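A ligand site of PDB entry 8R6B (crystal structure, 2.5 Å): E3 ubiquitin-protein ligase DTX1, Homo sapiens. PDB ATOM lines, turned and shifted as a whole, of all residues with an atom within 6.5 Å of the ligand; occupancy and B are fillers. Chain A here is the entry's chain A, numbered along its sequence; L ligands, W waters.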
ATOM      1  N   ARG A  17      31.809  -6.046  23.618  1.00  0.00           N
ATOM      2  CA  ARG A  17      32.104  -5.053  22.599  1.00  0.00           C
ATOM      3  C   ARG A  17      33.583  -5.123  22.238  1.00  0.00           C
ATOM      4  O   ARG A  17      34.442  -5.127  23.129  1.00  0.00           O
ATOM      5  CB  ARG A  17      31.752  -3.636  23.074  1.00  0.00           C
ATOM      6  CG  ARG A  17      30.418  -3.128  22.566  1.00  0.00           C
ATOM      7  CD  ARG A  17      30.136  -1.717  23.022  1.00  0.00           C
ATOM      8  NE  ARG A  17      30.375  -1.558  24.449  1.00  0.00           N
ATOM      9  CZ  ARG A  17      31.292  -0.751  24.973  1.00  0.00           C
ATOM     10  NH1 ARG A  17      32.057   0.014  24.211  1.00  0.00           N
ATOM     11  NH2 ARG A  17      31.453  -0.715  26.296  1.00  0.00           N
ATOM     12  N   ARG A  19      36.828  -3.600  21.389  1.00  0.00           N
ATOM     13  CA  ARG A  19      37.496  -2.335  21.622  1.00  0.00           C
ATOM     14  C   ARG A  19      38.810  -2.293  20.851  1.00  0.00           C
ATOM     15  O   ARG A  19      39.542  -3.283  20.835  1.00  0.00           O
ATOM     16  CB  ARG A  19      37.791  -2.140  23.114  1.00  0.00           C
ATOM     17  CG  ARG A  19      36.535  -2.056  23.972  1.00  0.00           C
ATOM     18  CD  ARG A  19      35.801  -0.771  23.701  1.00  0.00           C
ATOM     19  NE  ARG A  19      36.580   0.378  24.148  1.00  0.00           N
ATOM     20  CZ  ARG A  19      36.574   1.566  23.574  1.00  0.00           C
ATOM     21  NH1 ARG A  19      35.852   1.809  22.485  1.00  0.00           N
ATOM     22  NH2 ARG A  19      37.327   2.531  24.072  1.00  0.00           N
ATOM     23  N   TRP A  92      36.234  10.415  23.551  1.00  0.00           N
ATOM     24  CA  TRP A  92      35.376  10.986  24.581  1.00  0.00           C
ATOM     25  C   TRP A  92      36.065  10.888  25.932  1.00  0.00           C
ATOM     26  O   TRP A  92      36.828   9.953  26.188  1.00  0.00           O
ATOM     27  CB  TRP A  92      34.008  10.285  24.623  1.00  0.00           C
ATOM     28  CG  TRP A  92      34.090   8.806  24.838  1.00  0.00           C
ATOM     29  CD1 TRP A  92      34.241   7.848  23.881  1.00  0.00           C
ATOM     30  CD2 TRP A  92      34.019   8.109  26.096  1.00  0.00           C
ATOM     31  NE1 TRP A  92      34.277   6.597  24.458  1.00  0.00           N
ATOM     32  CE2 TRP A  92      34.142   6.736  25.814  1.00  0.00           C
ATOM     33  CE3 TRP A  92      33.868   8.518  27.426  1.00  0.00           C
ATOM     34  CZ2 TRP A  92      34.119   5.764  26.817  1.00  0.00           C
ATOM     35  CZ3 TRP A  92      33.849   7.556  28.419  1.00  0.00           C
ATOM     36  CH2 TRP A  92      33.971   6.195  28.107  1.00  0.00           C
ATOM     37  N   ASN A  94      36.298  10.330  29.822  1.00  0.00           N
ATOM     38  CA  ASN A  94      35.566   9.592  30.851  1.00  0.00           C
ATOM     39  C   ASN A  94      35.592  10.360  32.170  1.00  0.00           C
ATOM     40  O   ASN A  94      36.104  11.474  32.263  1.00  0.00           O
ATOM     41  CB  ASN A  94      36.104   8.161  30.973  1.00  0.00           C
ATOM     42  CG  ASN A  94      37.449   8.046  31.708  1.00  0.00           C
ATOM     43  OD1 ASN A  94      37.852   8.914  32.493  1.00  0.00           O
ATOM     44  ND2 ASN A  94      38.144   6.943  31.464  1.00  0.00           N
ATOM     45  N   ASP A  95      35.032   9.728  33.202  1.00  0.00           N
ATOM     46  CA  ASP A  95      34.914  10.381  34.509  1.00  0.00           C
ATOM     47  C   ASP A  95      36.287  10.688  35.104  1.00  0.00           C
ATOM     48  O   ASP A  95      36.464  11.720  35.765  1.00  0.00           O
ATOM     49  CB  ASP A  95      34.104   9.508  35.454  1.00  0.00           C
ATOM     50  CG  ASP A  95      32.684   9.272  34.966  1.00  0.00           C
ATOM     51  OD1 ASP A  95      32.050  10.258  34.516  1.00  0.00           O
ATOM     52  OD2 ASP A  95      32.202   8.131  35.038  1.00  0.00           O
ATOM     53  N   THR A 100      39.053   8.454  25.779  1.00  0.00           N
ATOM     54  CA  THR A 100      38.800   7.094  25.348  1.00  0.00           C
ATOM     55  C   THR A 100      38.249   7.113  23.927  1.00  0.00           C
ATOM     56  O   THR A 100      37.334   7.886  23.633  1.00  0.00           O
ATOM     57  CB  THR A 100      37.817   6.390  26.292  1.00  0.00           C
ATOM     58  OG1 THR A 100      38.224   6.602  27.652  1.00  0.00           O
ATOM     59  CG2 THR A 100      37.787   4.910  26.023  1.00  0.00           C
ATOM     60  N   ALA A 101      38.818   6.285  23.059  1.00  0.00           N
ATOM     61  CA  ALA A 101      38.344   6.230  21.679  1.00  0.00           C
ATOM     62  C   ALA A 101      37.047   5.450  21.585  1.00  0.00           C
ATOM     63  O   ALA A 101      36.848   4.450  22.274  1.00  0.00           O
ATOM     64  CB  ALA A 101      39.409   5.602  20.774  1.00  0.00           C
ATOM     65  N   TYR A 102      36.144   5.921  20.727  1.00  0.00           N
ATOM     66  CA  TYR A 102      34.923   5.196  20.433  1.00  0.00           C
ATOM     67  C   TYR A 102      35.252   3.864  19.757  1.00  0.00           C
ATOM     68  O   TYR A 102      36.361   3.649  19.252  1.00  0.00           O
ATOM     69  CB  TYR A 102      34.006   6.012  19.529  1.00  0.00           C
ATOM     70  CG  TYR A 102      33.384   7.221  20.179  1.00  0.00           C
ATOM     71  CD1 TYR A 102      34.018   8.459  20.144  1.00  0.00           C
ATOM     72  CD2 TYR A 102      32.151   7.144  20.818  1.00  0.00           C
ATOM     73  CE1 TYR A 102      33.450   9.582  20.735  1.00  0.00           C
ATOM     74  CE2 TYR A 102      31.570   8.251  21.409  1.00  0.00           C
ATOM     75  CZ  TYR A 102      32.226   9.470  21.366  1.00  0.00           C
ATOM     76  OH  TYR A 102      31.653  10.571  21.954  1.00  0.00           O
ATOM     77  N   ASP A 103      34.268   2.961  19.749  1.00  0.00           N
ATOM     78  CA  ASP A 103      34.371   1.779  18.906  1.00  0.00           C
ATOM     79  C   ASP A 103      34.635   2.203  17.470  1.00  0.00           C
ATOM     80  O   ASP A 103      34.191   3.266  17.024  1.00  0.00           O
ATOM     81  CB  ASP A 103      33.095   0.927  18.984  1.00  0.00           C
ATOM     82  CG  ASP A 103      32.850   0.354  20.371  1.00  0.00           C
ATOM     83  OD1 ASP A 103      33.825   0.208  21.136  1.00  0.00           O
ATOM     84  OD2 ASP A 103      31.685   0.046  20.673  1.00  0.00           O
ATOM     85  N   PHE A 128      23.982   2.768  20.467  1.00  0.00           N
ATOM     86  CA  PHE A 128      24.324   3.800  21.440  1.00  0.00           C
ATOM     87  C   PHE A 128      23.223   4.849  21.501  1.00  0.00           C
ATOM     88  O   PHE A 128      22.924   5.502  20.501  1.00  0.00           O
ATOM     89  CB  PHE A 128      25.658   4.446  21.085  1.00  0.00           C
ATOM     90  CG  PHE A 128      26.862   3.678  21.544  1.00  0.00           C
ATOM     91  CD1 PHE A 128      27.226   2.489  20.924  1.00  0.00           C
ATOM     92  CD2 PHE A 128      27.645   4.147  22.583  1.00  0.00           C
ATOM     93  CE1 PHE A 128      28.341   1.781  21.342  1.00  0.00           C
ATOM     94  CE2 PHE A 128      28.766   3.445  23.001  1.00  0.00           C
ATOM     95  CZ  PHE A 128      29.106   2.263  22.378  1.00  0.00           C
ATOM     96  N   TYR A 130      22.972   7.932  22.203  1.00  0.00           N
ATOM     97  CA  TYR A 130      23.727   9.162  22.387  1.00  0.00           C
ATOM     98  C   TYR A 130      23.602  10.047  21.158  1.00  0.00           C
ATOM     99  O   TYR A 130      23.346   9.571  20.051  1.00  0.00           O
ATOM    100  CB  TYR A 130      25.212   8.879  22.660  1.00  0.00           C
ATOM    101  CG  TYR A 130      25.484   8.256  24.007  1.00  0.00           C
ATOM    102  CD1 TYR A 130      25.622   9.050  25.143  1.00  0.00           C
ATOM    103  CD2 TYR A 130      25.618   6.872  24.149  1.00  0.00           C
ATOM    104  CE1 TYR A 130      25.874   8.489  26.379  1.00  0.00           C
ATOM    105  CE2 TYR A 130      25.870   6.311  25.385  1.00  0.00           C
ATOM    106  CZ  TYR A 130      26.001   7.110  26.493  1.00  0.00           C
ATOM    107  OH  TYR A 130      26.251   6.550  27.719  1.00  0.00           O
ATOM    108  N   GLN A 139      28.971  14.969  23.656  1.00  0.00           N
ATOM    109  CA  GLN A 139      28.126  13.801  23.496  1.00  0.00           C
ATOM    110  C   GLN A 139      27.064  13.830  24.577  1.00  0.00           C
ATOM    111  O   GLN A 139      27.384  14.063  25.744  1.00  0.00           O
ATOM    112  CB  GLN A 139      28.956  12.517  23.595  1.00  0.00           C
ATOM    113  CG  GLN A 139      28.176  11.292  24.026  1.00  0.00           C
ATOM    114  CD  GLN A 139      29.071  10.231  24.636  1.00  0.00           C
ATOM    115  OE1 GLN A 139      29.922   9.662  23.964  1.00  0.00           O
ATOM    116  NE2 GLN A 139      28.879   9.960  25.931  1.00  0.00           N
ATOM    117  N   MET A 140      25.810  13.607  24.204  1.00  0.00           N
ATOM    118  CA  MET A 140      24.697  13.732  25.126  1.00  0.00           C
ATOM    119  C   MET A 140      23.945  12.414  25.242  1.00  0.00           C
ATOM    120  O   MET A 140      23.590  11.804  24.235  1.00  0.00           O
ATOM    121  CB  MET A 140      23.735  14.832  24.677  1.00  0.00           C
ATOM    122  CG  MET A 140      22.660  15.152  25.693  1.00  0.00           C
ATOM    123  SD  MET A 140      21.194  15.882  24.931  1.00  0.00           S
ATOM    124  CE  MET A 140      20.950  17.333  25.948  1.00  0.00           C
ATOM    125  N   ASN A 141      23.707  11.983  26.482  1.00  0.00           N
ATOM    126  CA  ASN A 141      22.843  10.828  26.727  1.00  0.00           C
ATOM    127  C   ASN A 141      21.400  11.205  26.426  1.00  0.00           C
ATOM    128  O   ASN A 141      20.878  12.182  26.960  1.00  0.00           O
ATOM    129  CB  ASN A 141      22.985  10.370  28.186  1.00  0.00           C
ATOM    130  CG  ASN A 141      22.290   9.052  28.444  1.00  0.00           C
ATOM    131  OD1 ASN A 141      21.060   8.973  28.443  1.00  0.00           O
ATOM    132  ND2 ASN A 141      23.066   8.003  28.700  1.00  0.00           N
ATOM    133  N   THR A 144      19.149  10.910  29.875  1.00  0.00           N
ATOM    134  CA  THR A 144      19.459  11.759  31.016  1.00  0.00           C
ATOM    135  C   THR A 144      19.763  13.209  30.632  1.00  0.00           C
ATOM    136  O   THR A 144      19.737  14.072  31.519  1.00  0.00           O
ATOM    137  CB  THR A 144      20.656  11.210  31.784  1.00  0.00           C
ATOM    138  OG1 THR A 144      21.864  11.714  31.209  1.00  0.00           O
ATOM    139  CG2 THR A 144      20.666   9.696  31.719  1.00  0.00           C
ATOM    140  N   ARG A 145      20.049  13.483  29.365  1.00  0.00           N
ATOM    141  CA  ARG A 145      20.456  14.789  28.857  1.00  0.00           C
ATOM    142  C   ARG A 145      21.806  15.241  29.398  1.00  0.00           C
ATOM    143  O   ARG A 145      22.189  16.405  29.198  1.00  0.00           O
ATOM    144  CB  ARG A 145      19.408  15.873  29.150  1.00  0.00           C
ATOM    145  CG  ARG A 145      18.378  16.083  28.043  1.00  0.00           C
ATOM    146  CD  ARG A 145      17.286  15.023  28.028  1.00  0.00           C
ATOM    147  NE  ARG A 145      16.266  15.376  27.057  1.00  0.00           N
ATOM    148  CZ  ARG A 145      15.058  14.820  26.954  1.00  0.00           C
ATOM    149  NH1 ARG A 145      14.674  13.849  27.770  1.00  0.00           N
ATOM    150  NH2 ARG A 145      14.221  15.258  26.021  1.00  0.00           N
ATOM    151  N   ARG A 146      22.543  14.366  30.079  1.00  0.00           N
ATOM    152  CA  ARG A 146      23.881  14.707  30.553  1.00  0.00           C
ATOM    153  C   ARG A 146      24.887  14.567  29.426  1.00  0.00           C
ATOM    154  O   ARG A 146      24.706  13.793  28.483  1.00  0.00           O
ATOM    155  CB  ARG A 146      24.282  13.826  31.740  1.00  0.00           C
ATOM    156  CG  ARG A 146      23.394  13.993  32.965  1.00  0.00           C
ATOM    157  CD  ARG A 146      23.926  13.197  34.132  1.00  0.00           C
ATOM    158  NE  ARG A 146      23.091  13.344  35.329  1.00  0.00           N
ATOM    159  CZ  ARG A 146      22.179  12.470  35.714  1.00  0.00           C
ATOM    160  NH1 ARG A 146      21.977  11.342  35.055  1.00  0.00           N
ATOM    161  NH2 ARG A 146      21.460  12.723  36.804  1.00  0.00           N
ATOM    162  N   ARG A 147      25.973  15.338  29.523  1.00  0.00           N
ATOM    163  CA  ARG A 147      26.930  15.434  28.426  1.00  0.00           C
ATOM    164  C   ARG A 147      28.358  15.144  28.881  1.00  0.00           C
ATOM    165  O   ARG A 147      28.743  15.401  30.023  1.00  0.00           O
ATOM    166  CB  ARG A 147      26.875  16.814  27.770  1.00  0.00           C
ATOM    167  CG  ARG A 147      25.535  17.124  27.117  1.00  0.00           C
ATOM    168  CD  ARG A 147      25.674  18.163  26.021  1.00  0.00           C
ATOM    169  NE  ARG A 147      24.361  18.576  25.524  1.00  0.00           N
ATOM    170  CZ  ARG A 147      24.169  19.577  24.677  1.00  0.00           C
ATOM    171  NH1 ARG A 147      25.181  20.299  24.209  1.00  0.00           N
ATOM    172  NH2 ARG A 147      22.932  19.857  24.274  1.00  0.00           N
ATOM    173  N   ARG A 148      29.138  14.617  27.941  1.00  0.00           N
ATOM    174  CA  ARG A 148      30.590  14.482  28.058  1.00  0.00           C
ATOM    175  C   ARG A 148      31.255  15.229  26.912  1.00  0.00           C
ATOM    176  O   ARG A 148      30.656  15.438  25.859  1.00  0.00           O
ATOM    177  CB  ARG A 148      31.030  13.006  28.032  1.00  0.00           C
ATOM    178  CG  ARG A 148      30.796  12.263  29.326  1.00  0.00           C
ATOM    179  CD  ARG A 148      30.916  10.768  29.120  1.00  0.00           C
ATOM    180  NE  ARG A 148      30.380  10.045  30.267  1.00  0.00           N
ATOM    181  CZ  ARG A 148      31.122   9.491  31.207  1.00  0.00           C
ATOM    182  NH1 ARG A 148      32.438   9.482  31.129  1.00  0.00           N
ATOM    183  NH2 ARG A 148      30.529   8.939  32.260  1.00  0.00           N
HETATM  184  P1  LIG L   1      24.335   9.404  32.584  1.00  0.00           P
HETATM  185  O1  LIG L   1      23.449   8.181  32.436  1.00  0.00           O
HETATM  186  O2  LIG L   1      24.476   9.928  33.990  1.00  0.00           O
HETATM  187  O3  LIG L   1      24.135  10.451  31.516  1.00  0.00           O
HETATM  188  P2  LIG L   1      26.502   8.587  30.865  1.00  0.00           P
HETATM  189  O4  LIG L   1      25.439   8.529  29.797  1.00  0.00           O
HETATM  190  O5  LIG L   1      27.634   9.582  30.775  1.00  0.00           O
HETATM  191  O6  LIG L   1      25.807   8.815  32.310  1.00  0.00           O
HETATM  192  O7  LIG L   1      27.062   7.092  31.075  1.00  0.00           O
HETATM  193  C1  LIG L   1      27.890   6.841  32.208  1.00  0.00           C
HETATM  194  C2  LIG L   1      28.636   5.530  31.980  1.00  0.00           C
HETATM  195  O8  LIG L   1      28.649   5.165  30.590  1.00  0.00           O
HETATM  196  C3  LIG L   1      30.087   5.672  32.403  1.00  0.00           C
HETATM  197  O9  LIG L   1      30.522   4.487  33.084  1.00  0.00           O
HETATM  198  C4  LIG L   1      30.851   5.824  31.116  1.00  0.00           C
HETATM  199  O10 LIG L   1      32.126   5.175  31.261  1.00  0.00           O
HETATM  200  C5  LIG L   1      29.979   5.132  30.085  1.00  0.00           C
HETATM  201  N1  LIG L   1      30.079   5.800  28.752  1.00  0.00           N
HETATM  202  C6  LIG L   1      29.716   7.054  28.482  1.00  0.00           C
HETATM  203  N2  LIG L   1      29.948   7.370  27.194  1.00  0.00           N
HETATM  204  C7  LIG L   1      30.472   6.285  26.621  1.00  0.00           C
HETATM  205  C8  LIG L   1      30.962   5.895  25.278  1.00  0.00           C
HETATM  206  N3  LIG L   1      30.957   6.730  24.219  1.00  0.00           N
HETATM  207  N4  LIG L   1      31.435   4.667  25.083  1.00  0.00           N
HETATM  208  C9  LIG L   1      31.469   3.792  26.097  1.00  0.00           C
HETATM  209  N5  LIG L   1      31.060   4.045  27.345  1.00  0.00           N
HETATM  210  C10 LIG L   1      30.558   5.252  27.648  1.00  0.00           C
HETATM  211  O   HOH W   1      27.262  11.634  28.760  1.00  0.00           O
HETATM  212  O   HOH W   2      27.452  10.794  33.653  1.00  0.00           O
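Residues that only touch the ligand: Tyr 102 (3.3 Å) and Phe 128 (3.6 Å). Hydrophobic or aromatic side chains within 4 Å of the ligand: Trp 92, Tyr 102, Phe 128 and Tyr 130. Of the 19 residues printed, 9 come within 4 Å of the ligand. The nearest printed residue that does not touch the ligand is Asp 95 (4.2 Å).
An oxygen (O3) of the ligand is in hydrogen-bond range of the side-chain hydroxyl of Thr 144 (2.6 Å). An oxygen (O4) of the ligand lies within hydrogen-bond range of the side-chain amide nitrogen of Asn 141 (2.7 Å). The guanidinium group of Arg 148 lies within salt-bridge range of an oxygen (O5) of the ligand, 2.8 Å away. The side-chain hydroxyl (OH) of Tyr 130 is in hydrogen-bond range of an oxygen (O4) of the ligand (3.0 Å). NH1 of Arg 146 lies within salt-bridge range of O2 of the ligand. The side-chain amide nitrogen (NE2) of Gln 139 lies within hydrogen-bond range of a nitrogen (N2) of the ligand, 3.1 Å away. The indole nitrogen (NE1) of Trp 92 lies close to a nitrogen (N4) of the ligand, 3.5 Å away.
Water W1 bridges an oxygen (O5) of the ligand and the backbone carbonyl oxygen of Arg 146.
N of Thr 144 sits at hydrogen-bond distance from OD1 of Asn 141. OG1 of Thr 144 is in hydrogen-bond range of N of Arg 146 (3.0 Å). The backbone NH (N) of Asn 141 lies within hydrogen-bond range of the backbone carbonyl oxygen (O) of Arg 146 (2.9 Å). The backbone NH (N) of Gln 139 lies within hydrogen-bond range of the backbone carbonyl oxygen (O) of Arg 148, at 2.8 Å. The side-chain carboxylate of Asp 95 lies within salt-bridge range of the guanidinium group of Arg 148, 3.0 Å away. OE1 of Gln 139 is in hydrogen-bond range of OH of Tyr 102 (2.8 Å). The backbone NH (N) of Thr 100 is in hydrogen-bond range of the backbone carbonyl oxygen (O) of Trp 92, 2.7 Å away.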
